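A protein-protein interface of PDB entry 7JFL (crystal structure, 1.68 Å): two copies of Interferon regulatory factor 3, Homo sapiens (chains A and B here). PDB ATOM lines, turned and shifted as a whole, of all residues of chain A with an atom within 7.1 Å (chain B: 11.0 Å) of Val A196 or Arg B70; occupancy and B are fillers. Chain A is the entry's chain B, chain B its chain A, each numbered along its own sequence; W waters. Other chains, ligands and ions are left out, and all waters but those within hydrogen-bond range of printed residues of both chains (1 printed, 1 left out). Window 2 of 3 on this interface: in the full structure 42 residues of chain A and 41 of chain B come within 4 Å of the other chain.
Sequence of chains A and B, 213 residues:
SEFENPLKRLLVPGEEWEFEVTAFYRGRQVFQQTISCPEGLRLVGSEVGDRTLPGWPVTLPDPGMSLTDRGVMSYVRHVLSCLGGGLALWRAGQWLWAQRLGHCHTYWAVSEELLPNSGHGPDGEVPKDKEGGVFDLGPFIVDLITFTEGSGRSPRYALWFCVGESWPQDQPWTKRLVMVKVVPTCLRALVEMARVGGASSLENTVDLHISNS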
ATOM      1  N   LEU A 190      16.170 -21.368  -8.719  1.00  0.00           N
ATOM      2  CA  LEU A 190      16.678 -20.842  -9.981  1.00  0.00           C
ATOM      3  C   LEU A 190      16.013 -19.516 -10.334  1.00  0.00           C
ATOM      4  O   LEU A 190      16.674 -18.609 -10.857  1.00  0.00           O
ATOM      5  CB  LEU A 190      16.488 -21.866 -11.102  1.00  0.00           C
ATOM      6  CG  LEU A 190      17.464 -23.044 -11.091  1.00  0.00           C
ATOM      7  CD1 LEU A 190      16.936 -24.169 -11.966  1.00  0.00           C
ATOM      8  CD2 LEU A 190      18.838 -22.584 -11.575  1.00  0.00           C
ATOM      9  N   VAL A 191      14.713 -19.369 -10.042  1.00  0.00           N
ATOM     10  CA  VAL A 191      14.076 -18.076 -10.299  1.00  0.00           C
ATOM     11  C   VAL A 191      14.651 -17.013  -9.375  1.00  0.00           C
ATOM     12  O   VAL A 191      14.899 -15.879  -9.795  1.00  0.00           O
ATOM     13  CB  VAL A 191      12.544 -18.171 -10.156  1.00  0.00           C
ATOM     14  CG1 VAL A 191      11.914 -16.799 -10.325  1.00  0.00           C
ATOM     15  CG2 VAL A 191      11.980 -19.130 -11.164  1.00  0.00           C
ATOM     16  N   GLU A 192      14.862 -17.353  -8.109  1.00  0.00           N
ATOM     17  CA  GLU A 192      15.478 -16.402  -7.183  1.00  0.00           C
ATOM     18  C   GLU A 192      16.867 -15.989  -7.656  1.00  0.00           C
ATOM     19  O   GLU A 192      17.236 -14.810  -7.568  1.00  0.00           O
ATOM     20  CB  GLU A 192      15.540 -16.996  -5.780  1.00  0.00           C
ATOM     21  CG  GLU A 192      14.174 -17.054  -5.095  1.00  0.00           C
ATOM     22  CD  GLU A 192      13.604 -15.671  -4.763  1.00  0.00           C
ATOM     23  OE1 GLU A 192      13.956 -15.119  -3.697  1.00  0.00           O
ATOM     24  OE2 GLU A 192      12.799 -15.134  -5.560  1.00  0.00           O
ATOM     25  N   MET A 193      17.643 -16.941  -8.180  1.00  0.00           N
ATOM     26  CA  MET A 193      18.963 -16.609  -8.704  1.00  0.00           C
ATOM     27  C   MET A 193      18.864 -15.637  -9.874  1.00  0.00           C
ATOM     28  O   MET A 193      19.683 -14.722  -9.990  1.00  0.00           O
ATOM     29  CB  MET A 193      19.700 -17.889  -9.103  1.00  0.00           C
ATOM     30  CG  MET A 193      19.993 -18.775  -7.905  1.00  0.00           C
ATOM     31  SD  MET A 193      20.428 -20.476  -8.334  1.00  0.00           S
ATOM     32  CE  MET A 193      21.640 -20.168  -9.624  1.00  0.00           C
ATOM     33  N   ALA A 194      17.874 -15.820 -10.757  1.00  0.00           N
ATOM     34  CA  ALA A 194      17.691 -14.866 -11.852  1.00  0.00           C
ATOM     35  C   ALA A 194      17.364 -13.481 -11.314  1.00  0.00           C
ATOM     36  O   ALA A 194      17.835 -12.469 -11.843  1.00  0.00           O
ATOM     37  CB  ALA A 194      16.585 -15.341 -12.791  1.00  0.00           C
ATOM     38  N   ARG A 195      16.555 -13.414 -10.255  1.00  0.00           N
ATOM     39  CA  ARG A 195      16.231 -12.118  -9.669  1.00  0.00           C
ATOM     40  C   ARG A 195      17.459 -11.463  -9.050  1.00  0.00           C
ATOM     41  O   ARG A 195      17.673 -10.254  -9.212  1.00  0.00           O
ATOM     42  CB  ARG A 195      15.125 -12.277  -8.628  1.00  0.00           C
ATOM     43  CG  ARG A 195      13.775 -12.627  -9.233  1.00  0.00           C
ATOM     44  CD  ARG A 195      12.772 -12.992  -8.155  1.00  0.00           C
ATOM     45  NE  ARG A 195      11.458 -13.235  -8.739  1.00  0.00           N
ATOM     46  CZ  ARG A 195      10.604 -14.156  -8.305  1.00  0.00           C
ATOM     47  NH1 ARG A 195      10.941 -14.954  -7.286  1.00  0.00           N
ATOM     48  NH2 ARG A 195       9.426 -14.295  -8.904  1.00  0.00           N
ATOM     49  N   VAL A 196      18.258 -12.237  -8.301  1.00  0.00           N
ATOM     50  CA  VAL A 196      19.489 -11.703  -7.722  1.00  0.00           C
ATOM     51  C   VAL A 196      20.384 -11.149  -8.821  1.00  0.00           C
ATOM     52  O   VAL A 196      21.012 -10.090  -8.664  1.00  0.00           O
ATOM     53  CB  VAL A 196      20.208 -12.786  -6.893  1.00  0.00           C
ATOM     54  CG1 VAL A 196      21.579 -12.284  -6.421  1.00  0.00           C
ATOM     55  CG2 VAL A 196      19.363 -13.169  -5.699  1.00  0.00           C
ATOM     56  N   GLY A 197      20.428 -11.835  -9.962  1.00  0.00           N
ATOM     57  CA  GLY A 197      21.193 -11.365 -11.103  1.00  0.00           C
ATOM     58  C   GLY A 197      20.643 -10.119 -11.768  1.00  0.00           C
ATOM     59  O   GLY A 197      21.327  -9.547 -12.624  1.00  0.00           O
ATOM     60  N   GLY A 198      19.429  -9.700 -11.422  1.00  0.00           N
ATOM     61  CA  GLY A 198      18.877  -8.446 -11.917  1.00  0.00           C
ATOM     62  C   GLY A 198      17.609  -8.563 -12.738  1.00  0.00           C
ATOM     63  O   GLY A 198      17.117  -7.536 -13.230  1.00  0.00           O
ATOM     64  N   ALA A 199      17.044  -9.753 -12.919  1.00  0.00           N
ATOM     65  CA  ALA A 199      15.824  -9.903 -13.701  1.00  0.00           C
ATOM     66  C   ALA A 199      14.617  -9.451 -12.882  1.00  0.00           C
ATOM     67  O   ALA A 199      14.533  -9.734 -11.687  1.00  0.00           O
ATOM     68  CB  ALA A 199      15.650 -11.355 -14.136  1.00  0.00           C
ATOM     69  N   SER A 200      13.679  -8.763 -13.534  1.00  0.00           N
ATOM     70  CA  SER A 200      12.473  -8.264 -12.852  1.00  0.00           C
ATOM     71  C   SER A 200      11.199  -8.580 -13.636  1.00  0.00           C
ATOM     72  O   SER A 200      11.199  -8.578 -14.867  1.00  0.00           O
ATOM     73  CB  SER A 200      12.560  -6.753 -12.625  1.00  0.00           C
ATOM     74  OG  SER A 200      11.411  -6.267 -11.924  1.00  0.00           O
ATOM     75  N   LEU A 202       8.363  -6.885 -12.745  1.00  0.00           N
ATOM     76  CA  LEU A 202       7.475  -5.752 -12.446  1.00  0.00           C
ATOM     77  C   LEU A 202       6.943  -5.192 -13.761  1.00  0.00           C
ATOM     78  O   LEU A 202       7.700  -4.959 -14.698  1.00  0.00           O
ATOM     79  CB  LEU A 202       8.187  -4.668 -11.637  1.00  0.00           C
ATOM     80  CG  LEU A 202       7.316  -3.487 -11.163  1.00  0.00           C
ATOM     81  CD1 LEU A 202       6.102  -3.964 -10.385  1.00  0.00           C
ATOM     82  CD2 LEU A 202       8.158  -2.561 -10.310  1.00  0.00           C
ATOM     83  N   ARG B  26       4.243  -8.268  -3.104  1.00  0.00           N
ATOM     84  CA  ARG B  26       4.226  -9.012  -4.359  1.00  0.00           C
ATOM     85  C   ARG B  26       3.986 -10.499  -4.089  1.00  0.00           C
ATOM     86  O   ARG B  26       4.725 -11.385  -4.538  1.00  0.00           O
ATOM     87  CB  ARG B  26       5.528  -8.761  -5.137  1.00  0.00           C
ATOM     88  CG  ARG B  26       5.588  -9.335  -6.533  1.00  0.00           C
ATOM     89  CD  ARG B  26       4.876  -8.475  -7.543  1.00  0.00           C
ATOM     90  NE  ARG B  26       5.286  -8.810  -8.903  1.00  0.00           N
ATOM     91  CZ  ARG B  26       4.839  -8.185  -9.988  1.00  0.00           C
ATOM     92  NH1 ARG B  26       3.959  -7.203  -9.859  1.00  0.00           N
ATOM     93  NH2 ARG B  26       5.278  -8.528 -11.195  1.00  0.00           N
ATOM     94  N   ARG B  28       4.293 -12.364  -1.455  1.00  0.00           N
ATOM     95  CA  ARG B  28       5.193 -13.044  -0.530  1.00  0.00           C
ATOM     96  C   ARG B  28       4.951 -12.504   0.873  1.00  0.00           C
ATOM     97  O   ARG B  28       4.971 -11.287   1.077  1.00  0.00           O
ATOM     98  CB  ARG B  28       6.660 -12.825  -0.934  1.00  0.00           C
ATOM     99  CG  ARG B  28       7.664 -13.558  -0.041  1.00  0.00           C
ATOM    100  CD  ARG B  28       9.103 -13.462  -0.581  1.00  0.00           C
ATOM    101  NE  ARG B  28       9.203 -13.784  -2.006  1.00  0.00           N
ATOM    102  CZ  ARG B  28      10.350 -13.911  -2.673  1.00  0.00           C
ATOM    103  NH1 ARG B  28      11.507 -13.753  -2.044  1.00  0.00           N
ATOM    104  NH2 ARG B  28      10.342 -14.204  -3.969  1.00  0.00           N
ATOM    105  N   ASP B  62      11.903  -3.342   5.379  1.00  0.00           N
ATOM    106  CA  ASP B  62      12.533  -3.065   4.101  1.00  0.00           C
ATOM    107  C   ASP B  62      12.450  -4.311   3.223  1.00  0.00           C
ATOM    108  O   ASP B  62      12.748  -5.417   3.698  1.00  0.00           O
ATOM    109  CB  ASP B  62      13.993  -2.653   4.277  1.00  0.00           C
ATOM    110  CG  ASP B  62      14.644  -2.301   2.960  1.00  0.00           C
ATOM    111  OD1 ASP B  62      14.459  -1.157   2.489  1.00  0.00           O
ATOM    112  OD2 ASP B  62      15.320  -3.172   2.378  1.00  0.00           O
ATOM    113  N   PRO B  63      12.048  -4.183   1.957  1.00  0.00           N
ATOM    114  CA  PRO B  63      11.876  -5.381   1.117  1.00  0.00           C
ATOM    115  C   PRO B  63      13.172  -6.102   0.793  1.00  0.00           C
ATOM    116  O   PRO B  63      13.113  -7.224   0.278  1.00  0.00           O
ATOM    117  CB  PRO B  63      11.222  -4.825  -0.153  1.00  0.00           C
ATOM    118  CG  PRO B  63      11.668  -3.388  -0.198  1.00  0.00           C
ATOM    119  CD  PRO B  63      11.665  -2.948   1.243  1.00  0.00           C
ATOM    120  N   GLY B  64      14.334  -5.509   1.069  1.00  0.00           N
ATOM    121  CA  GLY B  64      15.575  -6.233   0.853  1.00  0.00           C
ATOM    122  C   GLY B  64      15.800  -7.378   1.812  1.00  0.00           C
ATOM    123  O   GLY B  64      16.709  -8.184   1.587  1.00  0.00           O
ATOM    124  N   MET B  65      14.998  -7.468   2.876  1.00  0.00           N
ATOM    125  CA  MET B  65      15.125  -8.580   3.809  1.00  0.00           C
ATOM    126  C   MET B  65      14.555  -9.859   3.222  1.00  0.00           C
ATOM    127  O   MET B  65      15.098 -10.946   3.452  1.00  0.00           O
ATOM    128  CB  MET B  65      14.420  -8.256   5.122  1.00  0.00           C
ATOM    129  CG  MET B  65      14.927  -7.004   5.801  1.00  0.00           C
ATOM    130  SD  MET B  65      16.653  -7.200   6.244  1.00  0.00           S
ATOM    131  CE  MET B  65      16.570  -8.594   7.374  1.00  0.00           C
ATOM    132  N   SER B  66      13.458  -9.750   2.462  1.00  0.00           N
ATOM    133  CA  SER B  66      12.730 -10.918   1.994  1.00  0.00           C
ATOM    134  C   SER B  66      12.609 -11.042   0.480  1.00  0.00           C
ATOM    135  O   SER B  66      12.318 -12.142   0.007  1.00  0.00           O
ATOM    136  CB  SER B  66      11.316 -10.938   2.594  1.00  0.00           C
ATOM    137  OG  SER B  66      11.377 -11.203   3.981  1.00  0.00           O
ATOM    138  N   LEU B  67      12.836  -9.979  -0.289  1.00  0.00           N
ATOM    139  CA  LEU B  67      12.681 -10.042  -1.736  1.00  0.00           C
ATOM    140  C   LEU B  67      14.035  -9.982  -2.431  1.00  0.00           C
ATOM    141  O   LEU B  67      15.051  -9.611  -1.836  1.00  0.00           O
ATOM    142  CB  LEU B  67      11.801  -8.904  -2.261  1.00  0.00           C
ATOM    143  CG  LEU B  67      10.385  -8.712  -1.709  1.00  0.00           C
ATOM    144  CD1 LEU B  67       9.639  -7.691  -2.554  1.00  0.00           C
ATOM    145  CD2 LEU B  67       9.625 -10.025  -1.631  1.00  0.00           C
ATOM    146  N   THR B  68      14.032 -10.343  -3.715  1.00  0.00           N
ATOM    147  CA  THR B  68      15.224 -10.271  -4.550  1.00  0.00           C
ATOM    148  C   THR B  68      14.994  -9.606  -5.906  1.00  0.00           C
ATOM    149  O   THR B  68      15.974  -9.253  -6.572  1.00  0.00           O
ATOM    150  CB  THR B  68      15.793 -11.680  -4.779  1.00  0.00           C
ATOM    151  OG1 THR B  68      14.761 -12.527  -5.300  1.00  0.00           O
ATOM    152  CG2 THR B  68      16.310 -12.273  -3.472  1.00  0.00           C
ATOM    153  N   ASP B  69      13.748  -9.436  -6.341  1.00  0.00           N
ATOM    154  CA  ASP B  69      13.443  -8.702  -7.567  1.00  0.00           C
ATOM    155  C   ASP B  69      13.706  -7.215  -7.328  1.00  0.00           C
ATOM    156  O   ASP B  69      12.948  -6.557  -6.614  1.00  0.00           O
ATOM    157  CB  ASP B  69      11.986  -8.966  -7.952  1.00  0.00           C
ATOM    158  CG  ASP B  69      11.548  -8.241  -9.222  1.00  0.00           C
ATOM    159  OD1 ASP B  69      11.949  -7.078  -9.446  1.00  0.00           O
ATOM    160  OD2 ASP B  69      10.753  -8.834  -9.979  1.00  0.00           O
ATOM    161  N   ARG B  70      14.757  -6.680  -7.955  1.00  0.00           N
ATOM    162  CA  ARG B  70      15.201  -5.324  -7.641  1.00  0.00           C
ATOM    163  C   ARG B  70      14.199  -4.262  -8.087  1.00  0.00           C
ATOM    164  O   ARG B  70      14.112  -3.199  -7.456  1.00  0.00           O
ATOM    165  CB  ARG B  70      16.561  -5.048  -8.281  1.00  0.00           C
ATOM    166  CG  ARG B  70      17.717  -5.828  -7.663  1.00  0.00           C
ATOM    167  CD  ARG B  70      18.920  -5.786  -8.602  1.00  0.00           C
ATOM    168  NE  ARG B  70      20.176  -6.112  -7.935  1.00  0.00           N
ATOM    169  CZ  ARG B  70      21.324  -6.321  -8.574  1.00  0.00           C
ATOM    170  NH1 ARG B  70      21.365  -6.251  -9.900  1.00  0.00           N
ATOM    171  NH2 ARG B  70      22.428  -6.606  -7.890  1.00  0.00           N
ATOM    172  N   GLY B  71      13.453  -4.514  -9.165  1.00  0.00           N
ATOM    173  CA  GLY B  71      12.427  -3.563  -9.574  1.00  0.00           C
ATOM    174  C   GLY B  71      11.285  -3.492  -8.575  1.00  0.00           C
ATOM    175  O   GLY B  71      10.857  -2.405  -8.170  1.00  0.00           O
ATOM    176  N   VAL B  72      10.796  -4.655  -8.137  1.00  0.00           N
ATOM    177  CA  VAL B  72       9.751  -4.683  -7.118  1.00  0.00           C
ATOM    178  C   VAL B  72      10.257  -4.060  -5.826  1.00  0.00           C
ATOM    179  O   VAL B  72       9.539  -3.299  -5.163  1.00  0.00           O
ATOM    180  CB  VAL B  72       9.258  -6.125  -6.889  1.00  0.00           C
ATOM    181  CG1 VAL B  72       8.322  -6.171  -5.687  1.00  0.00           C
ATOM    182  CG2 VAL B  72       8.574  -6.654  -8.140  1.00  0.00           C
ATOM    183  N   MET B  73      11.503  -4.363  -5.453  1.00  0.00           N
ATOM    184  CA  MET B  73      12.065  -3.802  -4.230  1.00  0.00           C
ATOM    185  C   MET B  73      12.085  -2.280  -4.290  1.00  0.00           C
ATOM    186  O   MET B  73      11.732  -1.611  -3.314  1.00  0.00           O
ATOM    187  CB  MET B  73      13.472  -4.345  -3.992  1.00  0.00           C
ATOM    188  CG  MET B  73      13.522  -5.776  -3.464  1.00  0.00           C
ATOM    189  SD  MET B  73      15.189  -6.481  -3.656  1.00  0.00           S
ATOM    190  CE  MET B  73      16.133  -5.292  -2.717  1.00  0.00           C
ATOM    191  N   SER B  74      12.482  -1.717  -5.439  1.00  0.00           N
ATOM    192  CA  SER B  74      12.514  -0.263  -5.585  1.00  0.00           C
ATOM    193  C   SER B  74      11.129   0.343  -5.391  1.00  0.00           C
ATOM    194  O   SER B  74      10.965   1.330  -4.662  1.00  0.00           O
ATOM    195  CB  SER B  74      13.072   0.115  -6.957  1.00  0.00           C
ATOM    196  OG  SER B  74      13.075   1.521  -7.130  1.00  0.00           O
ATOM    197  N   TYR B  75      10.118  -0.233  -6.041  1.00  0.00           N
ATOM    198  CA  TYR B  75       8.769   0.329  -5.953  1.00  0.00           C
ATOM    199  C   TYR B  75       8.174   0.156  -4.561  1.00  0.00           C
ATOM    200  O   TYR B  75       7.492   1.060  -4.056  1.00  0.00           O
ATOM    201  CB  TYR B  75       7.860  -0.305  -7.010  1.00  0.00           C
ATOM    202  CG  TYR B  75       7.891   0.443  -8.319  1.00  0.00           C
ATOM    203  CD1 TYR B  75       9.035   0.455  -9.104  1.00  0.00           C
ATOM    204  CD2 TYR B  75       6.785   1.164  -8.751  1.00  0.00           C
ATOM    205  CE1 TYR B  75       9.069   1.146 -10.298  1.00  0.00           C
ATOM    206  CE2 TYR B  75       6.809   1.854  -9.938  1.00  0.00           C
ATOM    207  CZ  TYR B  75       7.952   1.839 -10.706  1.00  0.00           C
ATOM    208  OH  TYR B  75       7.971   2.538 -11.879  1.00  0.00           O
ATOM    209  N   VAL B  76       8.398  -0.996  -3.928  1.00  0.00           N
ATOM    210  CA  VAL B  76       7.951  -1.164  -2.546  1.00  0.00           C
ATOM    211  C   VAL B  76       8.618  -0.131  -1.648  1.00  0.00           C
ATOM    212  O   VAL B  76       7.957   0.519  -0.832  1.00  0.00           O
ATOM    213  CB  VAL B  76       8.211  -2.597  -2.052  1.00  0.00           C
ATOM    214  CG1 VAL B  76       8.006  -2.690  -0.531  1.00  0.00           C
ATOM    215  CG2 VAL B  76       7.271  -3.570  -2.784  1.00  0.00           C
ATOM    216  N   ARG B  77       9.933   0.059  -1.803  1.00  0.00           N
ATOM    217  CA  ARG B  77      10.620   1.064  -0.998  1.00  0.00           C
ATOM    218  C   ARG B  77      10.012   2.442  -1.197  1.00  0.00           C
ATOM    219  O   ARG B  77       9.856   3.198  -0.232  1.00  0.00           O
ATOM    220  CB  ARG B  77      12.109   1.107  -1.336  1.00  0.00           C
ATOM    221  CG  ARG B  77      12.885  -0.023  -0.731  1.00  0.00           C
ATOM    222  CD  ARG B  77      14.368   0.118  -1.024  1.00  0.00           C
ATOM    223  NE  ARG B  77      15.121  -0.879  -0.276  1.00  0.00           N
ATOM    224  CZ  ARG B  77      15.935  -1.775  -0.823  1.00  0.00           C
ATOM    225  NH1 ARG B  77      16.134  -1.796  -2.138  1.00  0.00           N
ATOM    226  NH2 ARG B  77      16.564  -2.641  -0.045  1.00  0.00           N
ATOM    227  N   HIS B  78       9.647   2.777  -2.437  1.00  0.00           N
ATOM    228  CA  HIS B  78       9.017   4.069  -2.696  1.00  0.00           C
ATOM    229  C   HIS B  78       7.674   4.176  -1.973  1.00  0.00           C
ATOM    230  O   HIS B  78       7.388   5.182  -1.315  1.00  0.00           O
ATOM    231  CB  HIS B  78       8.848   4.283  -4.203  1.00  0.00           C
ATOM    232  CG  HIS B  78       8.314   5.633  -4.553  1.00  0.00           C
ATOM    233  ND1 HIS B  78       7.720   5.912  -5.765  1.00  0.00           N
ATOM    234  CD2 HIS B  78       8.294   6.787  -3.848  1.00  0.00           C
ATOM    235  CE1 HIS B  78       7.347   7.179  -5.785  1.00  0.00           C
ATOM    236  NE2 HIS B  78       7.674   7.727  -4.630  1.00  0.00           N
ATOM    237  N   LEU B 177       2.067  -4.489  -4.903  1.00  0.00           N
ATOM    238  CA  LEU B 177       3.330  -4.235  -4.223  1.00  0.00           C
ATOM    239  C   LEU B 177       3.218  -4.464  -2.723  1.00  0.00           C
ATOM    240  O   LEU B 177       4.091  -5.098  -2.116  1.00  0.00           O
ATOM    241  CB  LEU B 177       3.779  -2.802  -4.495  1.00  0.00           C
ATOM    242  CG  LEU B 177       4.126  -2.495  -5.940  1.00  0.00           C
ATOM    243  CD1 LEU B 177       4.332  -1.002  -6.075  1.00  0.00           C
ATOM    244  CD2 LEU B 177       5.361  -3.283  -6.352  1.00  0.00           C
HETATM  245  O   HOH W   1      10.644 -11.347 -10.512  1.00  0.00           O
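The side-chain hydroxyl (OG) of Ser A200 is in hydrogen-bond range of the side-chain carboxylate (OD1) of Asp B69, 2.7 Å away. The backbone carbonyl oxygen of Thr B68 lies close to the backbone carbonyl oxygen of Arg A195. The side-chain hydroxyl (OG1) of Thr B68 sits at hydrogen-bond distance from the side-chain carboxylate (OE1) of Glu A192 (3.2 Å). The guanidinium group (NH2) of Arg B28 is in salt-bridge range of the side-chain carboxylate (OE2) of Glu A192 (3.1 Å). The guanidinium group (NH1) of Arg A195 sits close to the guanidinium group (NH2) of Arg B28 (3.5 Å).
The side-chain carboxylate (OD1) of Asp B69 lies within hydrogen-bond range of the backbone NH (N) of Gly B71, 3.0 Å away. The side-chain carboxylate of Asp B69 is in hydrogen-bond range of the backbone NH of Val B72, at 3.0 Å. The side-chain hydroxyl (OG) of Ser A200 sits at hydrogen-bond distance from the backbone NH (N) of Leu A202. OE2 of Glu A192 is in salt-bridge range of NH1 of Arg A195. NH1 of Arg B28 is in hydrogen-bond range of O of Ser B66. N of Arg B26 sits at hydrogen-bond distance from O of Leu B177 (3.3 Å).
Among the printed residues, merely in contact across the chains: Arg A195 with Asp B69 (3.9 Å), Val A196 with Thr B68 (3.9 Å), Val A196 with Arg B70 (3.8 Å), Gly A198 with Arg B70 (3.9 Å), Ser A200 with Gly B71 (3.7 Å), Leu A202 with Arg B26 (3.8 Å), Leu A202 with Gly B71 (3.4 Å) and Leu A202 with Tyr B75 (3.4 Å).
Of the printed residues of chain B, Val A196 touches Thr B68 and Arg B70. Arg B70 touches just these residues of chain A: Val A196 (3.8 Å) and Gly A198 (3.9 Å). Of the printed residues of chain B, Glu A192 touches Arg B28 and Thr B68. Ala A194 touches none of the printed residues of chain B. No residue of chain B comes within 4 Å of Gly A197. No residue of chain B comes within 4 Å of Ala A199. Of the printed residues of chain B, Arg A195 touches Arg B28 (3.5 Å), Thr B68 (3.3 Å) and Asp B69 (3.9 Å). Of the printed residues of chain A, Tyr B75 touches Leu A202. Of the printed residues of chain A, Arg B26 touches Leu A202 (3.8 Å). Val B72 touches none of the printed residues of chain A.
Of the 12 printed residues of chain A, 6 touch a printed residue of chain B. Hydrophobic or aromatic side chains of chain A within 4 Å of the printed part of chain B: Val A196 and Leu A202. Of the 20 printed residues of chain B, 7 touch a printed residue of chain A. Hydrophobic or aromatic side chains of chain B within 4 Å of the printed part of chain A: Tyr B75.
No position is printed for both chains.
Water W1 bridges OD2 of Asp B69 and NE of Arg A195.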
